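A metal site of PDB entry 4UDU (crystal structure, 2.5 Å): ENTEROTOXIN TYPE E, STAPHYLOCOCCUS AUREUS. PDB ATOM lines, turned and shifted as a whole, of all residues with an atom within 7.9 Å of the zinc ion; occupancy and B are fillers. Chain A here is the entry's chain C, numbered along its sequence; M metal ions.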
ATOM      1  N   ASN A 128      26.475   5.966 -10.692  1.00  0.00           N
ATOM      2  CA  ASN A 128      26.503   7.410 -10.938  1.00  0.00           C
ATOM      3  C   ASN A 128      27.398   8.005  -9.849  1.00  0.00           C
ATOM      4  O   ASN A 128      26.971   8.165  -8.705  1.00  0.00           O
ATOM      5  CB  ASN A 128      25.087   7.999 -10.907  1.00  0.00           C
ATOM      6  CG  ASN A 128      24.134   7.414 -11.912  1.00  0.00           C
ATOM      7  OD1 ASN A 128      24.412   7.365 -13.120  1.00  0.00           O
ATOM      8  ND2 ASN A 128      22.970   6.998 -11.455  1.00  0.00           N
ATOM      9  N   TRP A 130      29.907  10.974  -8.290  1.00  0.00           N
ATOM     10  CA  TRP A 130      30.142  12.416  -8.190  1.00  0.00           C
ATOM     11  C   TRP A 130      31.289  12.679  -7.228  1.00  0.00           C
ATOM     12  O   TRP A 130      31.252  12.220  -6.085  1.00  0.00           O
ATOM     13  CB  TRP A 130      28.880  13.141  -7.677  1.00  0.00           C
ATOM     14  CG  TRP A 130      27.856  13.454  -8.727  1.00  0.00           C
ATOM     15  CD1 TRP A 130      27.817  14.547  -9.529  1.00  0.00           C
ATOM     16  CD2 TRP A 130      26.684  12.695  -9.013  1.00  0.00           C
ATOM     17  NE1 TRP A 130      26.700  14.509 -10.335  1.00  0.00           N
ATOM     18  CE2 TRP A 130      25.972  13.386 -10.024  1.00  0.00           C
ATOM     19  CE3 TRP A 130      26.157  11.491  -8.525  1.00  0.00           C
ATOM     20  CZ2 TRP A 130      24.785  12.908 -10.565  1.00  0.00           C
ATOM     21  CZ3 TRP A 130      24.949  11.033  -9.033  1.00  0.00           C
ATOM     22  CH2 TRP A 130      24.283  11.726 -10.052  1.00  0.00           C
ATOM     23  N   VAL A 185      24.136   5.452  -2.134  1.00  0.00           N
ATOM     24  CA  VAL A 185      22.683   5.392  -2.252  1.00  0.00           C
ATOM     25  C   VAL A 185      22.294   4.292  -3.239  1.00  0.00           C
ATOM     26  O   VAL A 185      22.701   4.331  -4.402  1.00  0.00           O
ATOM     27  CB  VAL A 185      22.072   6.772  -2.634  1.00  0.00           C
ATOM     28  CG1 VAL A 185      20.558   6.698  -2.776  1.00  0.00           C
ATOM     29  CG2 VAL A 185      22.446   7.858  -1.624  1.00  0.00           C
ATOM     30  N   PHE A 186      21.531   3.306  -2.754  1.00  0.00           N
ATOM     31  CA  PHE A 186      21.033   2.194  -3.559  1.00  0.00           C
ATOM     32  C   PHE A 186      19.612   2.580  -3.964  1.00  0.00           C
ATOM     33  O   PHE A 186      18.649   2.283  -3.257  1.00  0.00           O
ATOM     34  CB  PHE A 186      21.106   0.862  -2.779  1.00  0.00           C
ATOM     35  CG  PHE A 186      22.504   0.506  -2.306  1.00  0.00           C
ATOM     36  CD1 PHE A 186      22.983   0.975  -1.087  1.00  0.00           C
ATOM     37  CD2 PHE A 186      23.343  -0.281  -3.098  1.00  0.00           C
ATOM     38  CE1 PHE A 186      24.277   0.662  -0.676  1.00  0.00           C
ATOM     39  CE2 PHE A 186      24.631  -0.587  -2.664  1.00  0.00           C
ATOM     40  CZ  PHE A 186      25.090  -0.123  -1.453  1.00  0.00           C
ATOM     41  N   HIS A 187      19.515   3.335  -5.076  1.00  0.00           N
ATOM     42  CA  HIS A 187      18.265   3.882  -5.618  1.00  0.00           C
ATOM     43  C   HIS A 187      17.460   2.855  -6.402  1.00  0.00           C
ATOM     44  O   HIS A 187      17.928   2.335  -7.417  1.00  0.00           O
ATOM     45  CB  HIS A 187      18.562   5.135  -6.465  1.00  0.00           C
ATOM     46  CG  HIS A 187      17.451   6.141  -6.516  1.00  0.00           C
ATOM     47  ND1 HIS A 187      17.694   7.448  -6.925  1.00  0.00           N
ATOM     48  CD2 HIS A 187      16.144   6.021  -6.216  1.00  0.00           C
ATOM     49  CE1 HIS A 187      16.533   8.066  -6.851  1.00  0.00           C
ATOM     50  NE2 HIS A 187      15.561   7.244  -6.432  1.00  0.00           N
ATOM     51  N   SER A 188      16.236   2.573  -5.921  1.00  0.00           N
ATOM     52  CA  SER A 188      15.302   1.625  -6.555  1.00  0.00           C
ATOM     53  C   SER A 188      14.379   2.314  -7.576  1.00  0.00           C
ATOM     54  O   SER A 188      14.257   3.543  -7.564  1.00  0.00           O
ATOM     55  CB  SER A 188      14.488   0.895  -5.492  1.00  0.00           C
ATOM     56  OG  SER A 188      15.238  -0.151  -4.908  1.00  0.00           O
ATOM     57  N   GLY A 191      11.364   4.694  -6.175  1.00  0.00           N
ATOM     58  CA  GLY A 191      11.867   5.942  -5.609  1.00  0.00           C
ATOM     59  C   GLY A 191      12.446   5.764  -4.225  1.00  0.00           C
ATOM     60  O   GLY A 191      12.962   6.726  -3.647  1.00  0.00           O
ATOM     61  N   SER A 192      12.357   4.538  -3.678  1.00  0.00           N
ATOM     62  CA  SER A 192      12.874   4.171  -2.351  1.00  0.00           C
ATOM     63  C   SER A 192      14.399   4.100  -2.383  1.00  0.00           C
ATOM     64  O   SER A 192      14.984   3.616  -3.352  1.00  0.00           O
ATOM     65  CB  SER A 192      12.287   2.845  -1.898  1.00  0.00           C
ATOM     66  OG  SER A 192      12.632   1.787  -2.782  1.00  0.00           O
ATOM     67  N   THR A 193      15.056   4.602  -1.318  1.00  0.00           N
ATOM     68  CA  THR A 193      16.518   4.617  -1.222  1.00  0.00           C
ATOM     69  C   THR A 193      17.054   3.986   0.049  1.00  0.00           C
ATOM     70  O   THR A 193      16.453   4.112   1.119  1.00  0.00           O
ATOM     71  CB  THR A 193      17.064   6.054  -1.347  1.00  0.00           C
ATOM     72  OG1 THR A 193      16.559   6.864  -0.285  1.00  0.00           O
ATOM     73  CG2 THR A 193      16.766   6.703  -2.705  1.00  0.00           C
ATOM     74  N   LEU A 224      17.742  -1.070 -11.130  1.00  0.00           N
ATOM     75  CA  LEU A 224      18.455  -0.548  -9.966  1.00  0.00           C
ATOM     76  C   LEU A 224      19.787   0.073 -10.372  1.00  0.00           C
ATOM     77  O   LEU A 224      20.507  -0.469 -11.210  1.00  0.00           O
ATOM     78  CB  LEU A 224      18.678  -1.672  -8.932  1.00  0.00           C
ATOM     79  CG  LEU A 224      19.279  -1.260  -7.585  1.00  0.00           C
ATOM     80  CD1 LEU A 224      18.198  -0.933  -6.575  1.00  0.00           C
ATOM     81  CD2 LEU A 224      20.196  -2.340  -7.060  1.00  0.00           C
ATOM     82  N   HIS A 225      20.110   1.223  -9.750  1.00  0.00           N
ATOM     83  CA  HIS A 225      21.360   1.937  -9.956  1.00  0.00           C
ATOM     84  C   HIS A 225      21.913   2.428  -8.620  1.00  0.00           C
ATOM     85  O   HIS A 225      21.145   2.678  -7.682  1.00  0.00           O
ATOM     86  CB  HIS A 225      21.191   3.096 -10.961  1.00  0.00           C
ATOM     87  CG  HIS A 225      20.311   4.210 -10.472  1.00  0.00           C
ATOM     88  ND1 HIS A 225      18.943   4.190 -10.672  1.00  0.00           N
ATOM     89  CD2 HIS A 225      20.643   5.353  -9.827  1.00  0.00           C
ATOM     90  CE1 HIS A 225      18.494   5.315 -10.137  1.00  0.00           C
ATOM     91  NE2 HIS A 225      19.483   6.047  -9.620  1.00  0.00           N
ATOM     92  N   ILE A 226      23.235   2.574  -8.536  1.00  0.00           N
ATOM     93  CA  ILE A 226      23.913   3.049  -7.342  1.00  0.00           C
ATOM     94  C   ILE A 226      24.328   4.505  -7.545  1.00  0.00           C
ATOM     95  O   ILE A 226      25.021   4.824  -8.523  1.00  0.00           O
ATOM     96  CB  ILE A 226      25.106   2.130  -6.934  1.00  0.00           C
ATOM     97  CG1 ILE A 226      24.607   0.749  -6.450  1.00  0.00           C
ATOM     98  CG2 ILE A 226      26.008   2.788  -5.878  1.00  0.00           C
ATOM     99  CD1 ILE A 226      25.643  -0.389  -6.518  1.00  0.00           C
ATOM    100  N   ASP A 227      23.902   5.394  -6.640  1.00  0.00           N
ATOM    101  CA  ASP A 227      24.282   6.796  -6.652  1.00  0.00           C
ATOM    102  C   ASP A 227      25.385   6.961  -5.613  1.00  0.00           C
ATOM    103  O   ASP A 227      25.211   6.566  -4.459  1.00  0.00           O
ATOM    104  CB  ASP A 227      23.087   7.713  -6.374  1.00  0.00           C
ATOM    105  CG  ASP A 227      22.140   7.858  -7.551  1.00  0.00           C
ATOM    106  OD1 ASP A 227      22.577   8.379  -8.598  1.00  0.00           O
ATOM    107  OD2 ASP A 227      20.957   7.478  -7.417  1.00  0.00           O
ATOM    108  N   LEU A 228      26.539   7.489  -6.049  1.00  0.00           N
ATOM    109  CA  LEU A 228      27.691   7.692  -5.180  1.00  0.00           C
ATOM    110  C   LEU A 228      28.151   9.140  -5.174  1.00  0.00           C
ATOM    111  O   LEU A 228      28.386   9.721  -6.241  1.00  0.00           O
ATOM    112  CB  LEU A 228      28.845   6.756  -5.585  1.00  0.00           C
ATOM    113  CG  LEU A 228      28.926   5.420  -4.836  1.00  0.00           C
ATOM    114  CD1 LEU A 228      29.779   4.427  -5.589  1.00  0.00           C
ATOM    115  CD2 LEU A 228      29.483   5.613  -3.429  1.00  0.00           C
ATOM    116  N   TYR A 229      28.251   9.724  -3.979  1.00  0.00           N
ATOM    117  CA  TYR A 229      28.653  11.112  -3.781  1.00  0.00           C
ATOM    118  C   TYR A 229      29.876  11.161  -2.873  1.00  0.00           C
ATOM    119  O   TYR A 229      29.780  10.836  -1.685  1.00  0.00           O
ATOM    120  CB  TYR A 229      27.485  11.945  -3.194  1.00  0.00           C
ATOM    121  CG  TYR A 229      26.143  11.695  -3.840  1.00  0.00           C
ATOM    122  CD1 TYR A 229      25.734  12.411  -4.960  1.00  0.00           C
ATOM    123  CD2 TYR A 229      25.269  10.742  -3.313  1.00  0.00           C
ATOM    124  CE1 TYR A 229      24.489  12.179  -5.550  1.00  0.00           C
ATOM    125  CE2 TYR A 229      24.027  10.500  -3.894  1.00  0.00           C
ATOM    126  CZ  TYR A 229      23.635  11.217  -5.019  1.00  0.00           C
ATOM    127  OH  TYR A 229      22.417  10.983  -5.601  1.00  0.00           O
HETATM  128 ZN    ZN M   1      19.226   7.435  -8.213  1.00  0.00          ZN
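The backbone NH (N) of Asp 227 is in hydrogen-bond range of the backbone carbonyl oxygen (O) of Val 185, 2.8 Å away.
ND2 of Asn 128 is in hydrogen-bond range of OD1 of Asp 227, 3.2 Å away.
OD2 of Asp 227 binds the zinc ion.
NE2 of His 225 is bound to the zinc ion (2.0 Å).
The zinc ion is bound by ND1 of His 187 (2.0 Å).
The zinc ion has three donor atoms within binding distance.
Of the 15 residues printed, 3 come within 4 Å of the zinc ion.
The nearest printed residue that does not touch the zinc ion is Asn 128 (5.0 Å).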
